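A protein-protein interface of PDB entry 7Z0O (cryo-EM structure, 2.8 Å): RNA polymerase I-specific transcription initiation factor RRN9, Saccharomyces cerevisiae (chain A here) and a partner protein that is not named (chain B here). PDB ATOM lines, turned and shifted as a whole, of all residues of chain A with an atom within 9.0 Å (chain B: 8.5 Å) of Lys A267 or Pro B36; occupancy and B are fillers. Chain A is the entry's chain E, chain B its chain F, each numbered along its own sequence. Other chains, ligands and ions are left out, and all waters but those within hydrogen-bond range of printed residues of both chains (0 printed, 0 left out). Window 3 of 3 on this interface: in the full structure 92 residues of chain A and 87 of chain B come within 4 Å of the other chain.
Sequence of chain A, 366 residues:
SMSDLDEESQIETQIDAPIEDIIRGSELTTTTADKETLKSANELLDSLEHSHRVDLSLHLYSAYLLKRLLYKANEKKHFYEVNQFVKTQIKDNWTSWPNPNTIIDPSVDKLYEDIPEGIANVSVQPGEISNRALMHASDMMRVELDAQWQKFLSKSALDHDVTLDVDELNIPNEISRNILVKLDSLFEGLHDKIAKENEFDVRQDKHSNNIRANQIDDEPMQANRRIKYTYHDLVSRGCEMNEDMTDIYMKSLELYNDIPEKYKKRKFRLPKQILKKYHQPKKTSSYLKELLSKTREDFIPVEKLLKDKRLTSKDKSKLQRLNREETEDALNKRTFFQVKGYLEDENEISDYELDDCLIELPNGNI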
ATOM      1  N   SER A  62      10.199  -7.380   5.297  1.00  0.00           N
ATOM      2  CA  SER A  62      11.328  -8.304   5.285  1.00  0.00           C
ATOM      3  C   SER A  62      12.619  -7.587   4.919  1.00  0.00           C
ATOM      4  O   SER A  62      13.683  -7.887   5.471  1.00  0.00           O
ATOM      5  CB  SER A  62      11.055  -9.451   4.316  1.00  0.00           C
ATOM      6  OG  SER A  62      11.423  -9.099   2.995  1.00  0.00           O
ATOM      7  N   LEU A  65      13.701  -5.814   8.059  1.00  0.00           N
ATOM      8  CA  LEU A  65      14.229  -6.710   9.081  1.00  0.00           C
ATOM      9  C   LEU A  65      15.594  -7.258   8.690  1.00  0.00           C
ATOM     10  O   LEU A  65      16.445  -7.488   9.555  1.00  0.00           O
ATOM     11  CB  LEU A  65      13.250  -7.854   9.333  1.00  0.00           C
ATOM     12  CG  LEU A  65      12.143  -7.578  10.347  1.00  0.00           C
ATOM     13  CD1 LEU A  65      11.368  -8.848  10.632  1.00  0.00           C
ATOM     14  CD2 LEU A  65      12.724  -7.004  11.622  1.00  0.00           C
ATOM     15  N   LEU A  66      15.813  -7.494   7.396  1.00  0.00           N
ATOM     16  CA  LEU A  66      17.109  -7.992   6.948  1.00  0.00           C
ATOM     17  C   LEU A  66      18.211  -6.980   7.228  1.00  0.00           C
ATOM     18  O   LEU A  66      19.287  -7.334   7.722  1.00  0.00           O
ATOM     19  CB  LEU A  66      17.054  -8.328   5.460  1.00  0.00           C
ATOM     20  CG  LEU A  66      18.386  -8.740   4.837  1.00  0.00           C
ATOM     21  CD1 LEU A  66      18.928  -9.970   5.536  1.00  0.00           C
ATOM     22  CD2 LEU A  66      18.230  -8.992   3.350  1.00  0.00           C
ATOM     23  N   LYS A  67      17.958  -5.708   6.920  1.00  0.00           N
ATOM     24  CA  LYS A  67      18.971  -4.684   7.141  1.00  0.00           C
ATOM     25  C   LYS A  67      19.191  -4.437   8.626  1.00  0.00           C
ATOM     26  O   LYS A  67      20.329  -4.237   9.067  1.00  0.00           O
ATOM     27  CB  LYS A  67      18.573  -3.395   6.430  1.00  0.00           C
ATOM     28  CG  LYS A  67      18.601  -3.502   4.916  1.00  0.00           C
ATOM     29  CD  LYS A  67      18.731  -2.138   4.267  1.00  0.00           C
ATOM     30  CE  LYS A  67      17.422  -1.372   4.322  1.00  0.00           C
ATOM     31  NZ  LYS A  67      16.412  -1.933   3.386  1.00  0.00           N
ATOM     32  N   LEU A  69      18.608  -6.574  11.228  1.00  0.00           N
ATOM     33  CA  LEU A  69      19.233  -7.719  11.880  1.00  0.00           C
ATOM     34  C   LEU A  69      20.702  -7.842  11.497  1.00  0.00           C
ATOM     35  O   LEU A  69      21.533  -8.234  12.324  1.00  0.00           O
ATOM     36  CB  LEU A  69      18.480  -9.000  11.528  1.00  0.00           C
ATOM     37  CG  LEU A  69      17.471  -9.509  12.559  1.00  0.00           C
ATOM     38  CD1 LEU A  69      18.177  -9.897  13.846  1.00  0.00           C
ATOM     39  CD2 LEU A  69      16.402  -8.468  12.828  1.00  0.00           C
ATOM     40  N   LEU A  70      21.038  -7.530  10.245  1.00  0.00           N
ATOM     41  CA  LEU A  70      22.429  -7.607   9.811  1.00  0.00           C
ATOM     42  C   LEU A  70      23.301  -6.624  10.577  1.00  0.00           C
ATOM     43  O   LEU A  70      24.415  -6.964  10.993  1.00  0.00           O
ATOM     44  CB  LEU A  70      22.525  -7.348   8.309  1.00  0.00           C
ATOM     45  CG  LEU A  70      22.387  -8.567   7.400  1.00  0.00           C
ATOM     46  CD1 LEU A  70      22.273  -8.135   5.951  1.00  0.00           C
ATOM     47  CD2 LEU A  70      23.559  -9.506   7.590  1.00  0.00           C
ATOM     48  N   ALA A  73      23.714  -7.695  14.453  1.00  0.00           N
ATOM     49  CA  ALA A  73      24.606  -8.831  14.632  1.00  0.00           C
ATOM     50  C   ALA A  73      26.046  -8.522  14.248  1.00  0.00           C
ATOM     51  O   ALA A  73      26.940  -9.293  14.608  1.00  0.00           O
ATOM     52  CB  ALA A  73      24.102 -10.023  13.821  1.00  0.00           C
ATOM     53  N   ASN A  74      26.295  -7.420  13.535  1.00  0.00           N
ATOM     54  CA  ASN A  74      27.631  -7.129  13.034  1.00  0.00           C
ATOM     55  C   ASN A  74      28.022  -5.673  13.255  1.00  0.00           C
ATOM     56  O   ASN A  74      28.815  -5.121  12.485  1.00  0.00           O
ATOM     57  CB  ASN A  74      27.743  -7.468  11.548  1.00  0.00           C
ATOM     58  CG  ASN A  74      27.309  -8.882  11.241  1.00  0.00           C
ATOM     59  OD1 ASN A  74      28.095  -9.820  11.339  1.00  0.00           O
ATOM     60  ND2 ASN A  74      26.045  -9.044  10.872  1.00  0.00           N
ATOM     61  N   ILE A  90      22.505  -4.763  -0.806  1.00  0.00           N
ATOM     62  CA  ILE A  90      21.105  -4.375  -0.564  1.00  0.00           C
ATOM     63  C   ILE A  90      21.070  -2.857  -0.684  1.00  0.00           C
ATOM     64  O   ILE A  90      21.060  -2.113   0.298  1.00  0.00           O
ATOM     65  CB  ILE A  90      20.590  -4.874   0.787  1.00  0.00           C
ATOM     66  CG1 ILE A  90      21.168  -6.251   1.104  1.00  0.00           C
ATOM     67  CG2 ILE A  90      19.073  -4.913   0.792  1.00  0.00           C
ATOM     68  CD1 ILE A  90      21.074  -6.627   2.559  1.00  0.00           C
ATOM     69  N   LYS A 262      12.782 -10.159  19.046  1.00  0.00           N
ATOM     70  CA  LYS A 262      12.530 -11.589  19.178  1.00  0.00           C
ATOM     71  C   LYS A 262      13.548 -12.427  18.418  1.00  0.00           C
ATOM     72  O   LYS A 262      13.862 -13.540  18.851  1.00  0.00           O
ATOM     73  CB  LYS A 262      11.118 -11.920  18.693  1.00  0.00           C
ATOM     74  CG  LYS A 262      10.008 -11.238  19.479  1.00  0.00           C
ATOM     75  CD  LYS A 262       9.697 -11.983  20.769  1.00  0.00           C
ATOM     76  CE  LYS A 262      10.258 -11.259  21.982  1.00  0.00           C
ATOM     77  NZ  LYS A 262       9.888 -11.940  23.253  1.00  0.00           N
ATOM     78  N   TYR A 263      14.065 -11.919  17.303  1.00  0.00           N
ATOM     79  CA  TYR A 263      15.030 -12.661  16.507  1.00  0.00           C
ATOM     80  C   TYR A 263      16.336 -12.844  17.271  1.00  0.00           C
ATOM     81  O   TYR A 263      16.739 -11.999  18.074  1.00  0.00           O
ATOM     82  CB  TYR A 263      15.302 -11.933  15.193  1.00  0.00           C
ATOM     83  CG  TYR A 263      14.337 -12.269  14.082  1.00  0.00           C
ATOM     84  CD1 TYR A 263      14.486 -13.428  13.336  1.00  0.00           C
ATOM     85  CD2 TYR A 263      13.282 -11.423  13.776  1.00  0.00           C
ATOM     86  CE1 TYR A 263      13.610 -13.737  12.318  1.00  0.00           C
ATOM     87  CE2 TYR A 263      12.400 -11.723  12.758  1.00  0.00           C
ATOM     88  CZ  TYR A 263      12.569 -12.882  12.033  1.00  0.00           C
ATOM     89  OH  TYR A 263      11.694 -13.191  11.017  1.00  0.00           O
ATOM     90  N   LYS A 264      17.003 -13.966  17.011  1.00  0.00           N
ATOM     91  CA  LYS A 264      18.303 -14.251  17.602  1.00  0.00           C
ATOM     92  C   LYS A 264      19.393 -13.780  16.647  1.00  0.00           C
ATOM     93  O   LYS A 264      19.474 -14.253  15.508  1.00  0.00           O
ATOM     94  CB  LYS A 264      18.453 -15.741  17.899  1.00  0.00           C
ATOM     95  CG  LYS A 264      17.473 -16.272  18.931  1.00  0.00           C
ATOM     96  CD  LYS A 264      17.836 -15.816  20.332  1.00  0.00           C
ATOM     97  CE  LYS A 264      16.784 -14.872  20.893  1.00  0.00           C
ATOM     98  NZ  LYS A 264      17.065 -14.504  22.308  1.00  0.00           N
ATOM     99  N   LYS A 265      20.231 -12.853  17.114  1.00  0.00           N
ATOM    100  CA  LYS A 265      21.247 -12.255  16.256  1.00  0.00           C
ATOM    101  C   LYS A 265      22.319 -13.250  15.829  1.00  0.00           C
ATOM    102  O   LYS A 265      23.015 -12.997  14.841  1.00  0.00           O
ATOM    103  CB  LYS A 265      21.898 -11.071  16.967  1.00  0.00           C
ATOM    104  CG  LYS A 265      20.963  -9.902  17.200  1.00  0.00           C
ATOM    105  CD  LYS A 265      21.193  -9.290  18.569  1.00  0.00           C
ATOM    106  CE  LYS A 265      22.638  -8.860  18.746  1.00  0.00           C
ATOM    107  NZ  LYS A 265      22.881  -7.512  18.169  1.00  0.00           N
ATOM    108  N   ARG A 266      22.468 -14.366  16.545  1.00  0.00           N
ATOM    109  CA  ARG A 266      23.504 -15.336  16.201  1.00  0.00           C
ATOM    110  C   ARG A 266      23.309 -15.901  14.801  1.00  0.00           C
ATOM    111  O   ARG A 266      24.286 -16.250  14.131  1.00  0.00           O
ATOM    112  CB  ARG A 266      23.525 -16.464  17.232  1.00  0.00           C
ATOM    113  CG  ARG A 266      24.820 -17.252  17.266  1.00  0.00           C
ATOM    114  CD  ARG A 266      24.795 -18.586  18.056  1.00  0.00           C
ATOM    115  NE  ARG A 266      24.506 -18.505  19.489  1.00  0.00           N
ATOM    116  CZ  ARG A 266      23.336 -18.219  20.046  1.00  0.00           C
ATOM    117  NH1 ARG A 266      22.226 -18.126  19.333  1.00  0.00           N
ATOM    118  NH2 ARG A 266      23.268 -18.074  21.367  1.00  0.00           N
ATOM    119  N   LYS A 267      22.063 -15.996  14.341  1.00  0.00           N
ATOM    120  CA  LYS A 267      21.774 -16.499  13.005  1.00  0.00           C
ATOM    121  C   LYS A 267      22.174 -15.530  11.902  1.00  0.00           C
ATOM    122  O   LYS A 267      22.277 -15.947  10.744  1.00  0.00           O
ATOM    123  CB  LYS A 267      20.284 -16.820  12.881  1.00  0.00           C
ATOM    124  CG  LYS A 267      19.818 -17.966  13.760  1.00  0.00           C
ATOM    125  CD  LYS A 267      18.335 -18.235  13.568  1.00  0.00           C
ATOM    126  CE  LYS A 267      17.498 -17.121  14.178  1.00  0.00           C
ATOM    127  NZ  LYS A 267      16.038 -17.404  14.101  1.00  0.00           N
ATOM    128  N   PHE A 268      22.401 -14.257  12.226  1.00  0.00           N
ATOM    129  CA  PHE A 268      22.655 -13.232  11.222  1.00  0.00           C
ATOM    130  C   PHE A 268      24.089 -12.717  11.259  1.00  0.00           C
ATOM    131  O   PHE A 268      24.346 -11.579  10.856  1.00  0.00           O
ATOM    132  CB  PHE A 268      21.667 -12.079  11.390  1.00  0.00           C
ATOM    133  CG  PHE A 268      20.269 -12.422  10.970  1.00  0.00           C
ATOM    134  CD1 PHE A 268      19.399 -13.039  11.853  1.00  0.00           C
ATOM    135  CD2 PHE A 268      19.828 -12.141   9.690  1.00  0.00           C
ATOM    136  CE1 PHE A 268      18.117 -13.362  11.468  1.00  0.00           C
ATOM    137  CE2 PHE A 268      18.546 -12.460   9.302  1.00  0.00           C
ATOM    138  CZ  PHE A 268      17.690 -13.072  10.191  1.00  0.00           C
ATOM    139  N   ARG A 269      25.027 -13.528  11.737  1.00  0.00           N
ATOM    140  CA  ARG A 269      26.432 -13.155  11.679  1.00  0.00           C
ATOM    141  C   ARG A 269      26.967 -13.362  10.269  1.00  0.00           C
ATOM    142  O   ARG A 269      26.694 -14.380   9.627  1.00  0.00           O
ATOM    143  CB  ARG A 269      27.243 -13.977  12.677  1.00  0.00           C
ATOM    144  CG  ARG A 269      27.075 -13.534  14.116  1.00  0.00           C
ATOM    145  CD  ARG A 269      28.263 -13.947  14.961  1.00  0.00           C
ATOM    146  NE  ARG A 269      28.202 -15.351  15.346  1.00  0.00           N
ATOM    147  CZ  ARG A 269      28.142 -15.782  16.597  1.00  0.00           C
ATOM    148  NH1 ARG A 269      28.124 -14.941  17.618  1.00  0.00           N
ATOM    149  NH2 ARG A 269      28.100 -17.091  16.830  1.00  0.00           N
ATOM    150  N   LEU A 270      27.726 -12.386   9.784  1.00  0.00           N
ATOM    151  CA  LEU A 270      28.271 -12.476   8.439  1.00  0.00           C
ATOM    152  C   LEU A 270      29.263 -13.635   8.348  1.00  0.00           C
ATOM    153  O   LEU A 270      30.051 -13.853   9.273  1.00  0.00           O
ATOM    154  CB  LEU A 270      28.958 -11.170   8.050  1.00  0.00           C
ATOM    155  CG  LEU A 270      28.057 -10.097   7.437  1.00  0.00           C
ATOM    156  CD1 LEU A 270      28.869  -8.872   7.055  1.00  0.00           C
ATOM    157  CD2 LEU A 270      27.311 -10.647   6.234  1.00  0.00           C
ATOM    158  N   PRO A 271      29.245 -14.394   7.257  1.00  0.00           N
ATOM    159  CA  PRO A 271      30.182 -15.512   7.116  1.00  0.00           C
ATOM    160  C   PRO A 271      31.596 -15.015   6.855  1.00  0.00           C
ATOM    161  O   PRO A 271      31.833 -13.856   6.509  1.00  0.00           O
ATOM    162  CB  PRO A 271      29.630 -16.289   5.921  1.00  0.00           C
ATOM    163  CG  PRO A 271      28.899 -15.271   5.122  1.00  0.00           C
ATOM    164  CD  PRO A 271      28.340 -14.277   6.101  1.00  0.00           C
ATOM    165  N   ASP B  24      11.443 -12.372  -2.105  1.00  0.00           N
ATOM    166  CA  ASP B  24      12.348 -12.969  -1.130  1.00  0.00           C
ATOM    167  C   ASP B  24      13.493 -13.685  -1.836  1.00  0.00           C
ATOM    168  O   ASP B  24      14.655 -13.570  -1.433  1.00  0.00           O
ATOM    169  CB  ASP B  24      11.554 -13.912  -0.213  1.00  0.00           C
ATOM    170  CG  ASP B  24      12.434 -14.775   0.699  1.00  0.00           C
ATOM    171  OD1 ASP B  24      13.421 -15.394   0.251  1.00  0.00           O
ATOM    172  OD2 ASP B  24      12.118 -14.836   1.905  1.00  0.00           O
ATOM    173  N   LEU B  27      15.945 -11.126  -3.318  1.00  0.00           N
ATOM    174  CA  LEU B  27      16.806 -10.556  -2.289  1.00  0.00           C
ATOM    175  C   LEU B  27      17.841 -11.567  -1.806  1.00  0.00           C
ATOM    176  O   LEU B  27      18.984 -11.200  -1.516  1.00  0.00           O
ATOM    177  CB  LEU B  27      15.960 -10.049  -1.123  1.00  0.00           C
ATOM    178  CG  LEU B  27      16.623  -9.038  -0.189  1.00  0.00           C
ATOM    179  CD1 LEU B  27      17.318  -7.953  -0.986  1.00  0.00           C
ATOM    180  CD2 LEU B  27      15.596  -8.440   0.752  1.00  0.00           C
ATOM    181  N   ALA B  28      17.456 -12.842  -1.708  1.00  0.00           N
ATOM    182  CA  ALA B  28      18.393 -13.865  -1.249  1.00  0.00           C
ATOM    183  C   ALA B  28      19.547 -14.044  -2.227  1.00  0.00           C
ATOM    184  O   ALA B  28      20.703 -14.174  -1.810  1.00  0.00           O
ATOM    185  CB  ALA B  28      17.663 -15.190  -1.035  1.00  0.00           C
ATOM    186  N   ILE B  31      22.167 -11.151  -2.158  1.00  0.00           N
ATOM    187  CA  ILE B  31      23.189 -11.206  -1.123  1.00  0.00           C
ATOM    188  C   ILE B  31      23.947 -12.526  -1.148  1.00  0.00           C
ATOM    189  O   ILE B  31      24.698 -12.822  -0.214  1.00  0.00           O
ATOM    190  CB  ILE B  31      22.585 -10.953   0.268  1.00  0.00           C
ATOM    191  CG1 ILE B  31      21.748 -12.152   0.712  1.00  0.00           C
ATOM    192  CG2 ILE B  31      21.736  -9.700   0.257  1.00  0.00           C
ATOM    193  CD1 ILE B  31      21.451 -12.170   2.188  1.00  0.00           C
ATOM    194  N   ASN B  33      22.873 -15.430  -0.640  1.00  0.00           N
ATOM    195  CA  ASN B  33      22.381 -16.299   0.431  1.00  0.00           C
ATOM    196  C   ASN B  33      23.329 -16.306   1.627  1.00  0.00           C
ATOM    197  O   ASN B  33      23.559 -17.341   2.254  1.00  0.00           O
ATOM    198  CB  ASN B  33      22.142 -17.721  -0.079  1.00  0.00           C
ATOM    199  CG  ASN B  33      21.271 -17.757  -1.318  1.00  0.00           C
ATOM    200  OD1 ASN B  33      21.566 -17.101  -2.318  1.00  0.00           O
ATOM    201  ND2 ASN B  33      20.191 -18.525  -1.260  1.00  0.00           N
ATOM    202  N   ALA B  34      23.890 -15.138   1.945  1.00  0.00           N
ATOM    203  CA  ALA B  34      24.801 -15.043   3.080  1.00  0.00           C
ATOM    204  C   ALA B  34      24.078 -15.302   4.396  1.00  0.00           C
ATOM    205  O   ALA B  34      24.593 -16.017   5.264  1.00  0.00           O
ATOM    206  CB  ALA B  34      25.475 -13.674   3.099  1.00  0.00           C
ATOM    207  N   VAL B  35      22.890 -14.731   4.564  1.00  0.00           N
ATOM    208  CA  VAL B  35      22.114 -14.881   5.792  1.00  0.00           C
ATOM    209  C   VAL B  35      20.683 -15.258   5.427  1.00  0.00           C
ATOM    210  O   VAL B  35      20.238 -14.966   4.308  1.00  0.00           O
ATOM    211  CB  VAL B  35      22.153 -13.597   6.637  1.00  0.00           C
ATOM    212  CG1 VAL B  35      23.569 -13.295   7.087  1.00  0.00           C
ATOM    213  CG2 VAL B  35      21.591 -12.434   5.849  1.00  0.00           C
ATOM    214  N   PRO B  36      19.941 -15.919   6.313  1.00  0.00           N
ATOM    215  CA  PRO B  36      18.532 -16.209   6.019  1.00  0.00           C
ATOM    216  C   PRO B  36      17.723 -14.929   5.870  1.00  0.00           C
ATOM    217  O   PRO B  36      17.964 -13.936   6.556  1.00  0.00           O
ATOM    218  CB  PRO B  36      18.075 -17.025   7.234  1.00  0.00           C
ATOM    219  CG  PRO B  36      19.328 -17.553   7.838  1.00  0.00           C
ATOM    220  CD  PRO B  36      20.374 -16.520   7.585  1.00  0.00           C
ATOM    221  N   ILE B  37      16.754 -14.962   4.961  1.00  0.00           N
ATOM    222  CA  ILE B  37      15.871 -13.821   4.737  1.00  0.00           C
ATOM    223  C   ILE B  37      14.776 -13.833   5.797  1.00  0.00           C
ATOM    224  O   ILE B  37      14.033 -14.819   5.910  1.00  0.00           O
ATOM    225  CB  ILE B  37      15.274 -13.842   3.323  1.00  0.00           C
ATOM    226  CG1 ILE B  37      16.387 -13.781   2.278  1.00  0.00           C
ATOM    227  CG2 ILE B  37      14.317 -12.681   3.139  1.00  0.00           C
ATOM    228  CD1 ILE B  37      17.192 -12.508   2.323  1.00  0.00           C
ATOM    229  N   PRO B  38      14.637 -12.773   6.590  1.00  0.00           N
ATOM    230  CA  PRO B  38      13.639 -12.740   7.679  1.00  0.00           C
ATOM    231  C   PRO B  38      12.229 -12.393   7.207  1.00  0.00           C
ATOM    232  O   PRO B  38      11.776 -11.249   7.229  1.00  0.00           O
ATOM    233  CB  PRO B  38      14.206 -11.670   8.614  1.00  0.00           C
ATOM    234  CG  PRO B  38      14.909 -10.734   7.701  1.00  0.00           C
ATOM    235  CD  PRO B  38      15.450 -11.546   6.554  1.00  0.00           C
ATOM    236  N   PHE B  39      11.505 -13.412   6.758  1.00  0.00           N
ATOM    237  CA  PHE B  39      10.128 -13.241   6.317  1.00  0.00           C
ATOM    238  C   PHE B  39       9.176 -13.518   7.473  1.00  0.00           C
ATOM    239  O   PHE B  39       9.276 -14.555   8.134  1.00  0.00           O
ATOM    240  CB  PHE B  39       9.811 -14.167   5.144  1.00  0.00           C
ATOM    241  CG  PHE B  39       8.689 -13.679   4.279  1.00  0.00           C
ATOM    242  CD1 PHE B  39       7.374 -13.925   4.626  1.00  0.00           C
ATOM    243  CD2 PHE B  39       8.949 -12.968   3.120  1.00  0.00           C
ATOM    244  CE1 PHE B  39       6.339 -13.475   3.833  1.00  0.00           C
ATOM    245  CE2 PHE B  39       7.917 -12.516   2.323  1.00  0.00           C
ATOM    246  CZ  PHE B  39       6.612 -12.770   2.680  1.00  0.00           C
ATOM    247  N   LYS B  40       8.254 -12.587   7.709  1.00  0.00           N
ATOM    248  CA  LYS B  40       7.277 -12.692   8.789  1.00  0.00           C
ATOM    249  C   LYS B  40       5.886 -12.511   8.197  1.00  0.00           C
ATOM    250  O   LYS B  40       5.548 -11.425   7.719  1.00  0.00           O
ATOM    251  CB  LYS B  40       7.548 -11.652   9.875  1.00  0.00           C
ATOM    252  CG  LYS B  40       8.395 -12.162  11.027  1.00  0.00           C
ATOM    253  CD  LYS B  40       7.594 -13.060  11.947  1.00  0.00           C
ATOM    254  CE  LYS B  40       7.861 -12.731  13.403  1.00  0.00           C
ATOM    255  NZ  LYS B  40       9.241 -13.107  13.806  1.00  0.00           N
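Of the 12 printed residues of chain B, 7 touch a printed residue of chain A.
Of the 19 printed residues of chain A, 8 touch a printed residue of chain B.
Printed residues of chain A that touch a printed residue of chain B: Ser A62, Leu A65, Leu A66, Leu A70, Ile A90, Tyr A263, Lys A267 and Phe A268.
Hydrophobic or aromatic side chains of chain A that line the printed part of chain B: Leu A65, Leu A66, Leu A70, Ile A90, Tyr A263 and Phe A268.
Along chain A the printed residues that touch a printed residue of chain B span positions 62 to 268.
Among the printed residues, 13 pairs touch across the chains.
Among the printed residues, no Asp or Glu carboxylate lies within 4 Å of a Lys or Arg side-chain nitrogen of the other chain.
Of chain B, only Pro B36 comes within 4 Å of Lys A267.
Printed residues of chain A within 4 Å of Pro B36: Lys A267 and Phe A268.
Of chain A, only Leu A66 (3.6 Å) and Leu A70 (3.8 Å) come within 4 Å of Val B35.
Ile B37 touches just one residue of chain A: Leu A66.
Of the printed residues of chain B, Phe A268 touches Pro B36.
Printed residues of chain B within 4 Å of Ser A62: Pro B38.
Ala B28 touches none of the printed residues of chain A.
The nearest residue of chain B that does not touch Lys A267 is Val B35 (4.7 Å).
The nearest printed residue of chain B that does not touch Ile A90 is Val B35 (6.7 Å).
Ser A62 touches Pro B38.
Pro B38 touches Leu A65.
Leu A66 touches Leu B27.
CD2 of Leu A66 touches CD1 of Ile B37, 3.8 Å away.
Val B35 touches Leu A70.
CG2 of Ile A90 touches CD1 of Leu B27, at 3.9 Å.
Ile B31 touches Ile A90 (CG2 to CG1, 3.6 Å).
Pro B38 touches Tyr A263.
CG of Lys B40 touches OH of Tyr A263, at 3.5 Å.
Phe A268 touches Pro B36.
The backbone carbonyl oxygen of Leu A70 sits at hydrogen-bond distance from the side-chain amide nitrogen of Asn A74 (2.6 Å).
O of Phe A268 lies within hydrogen-bond range of ND2 of Asn A74.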
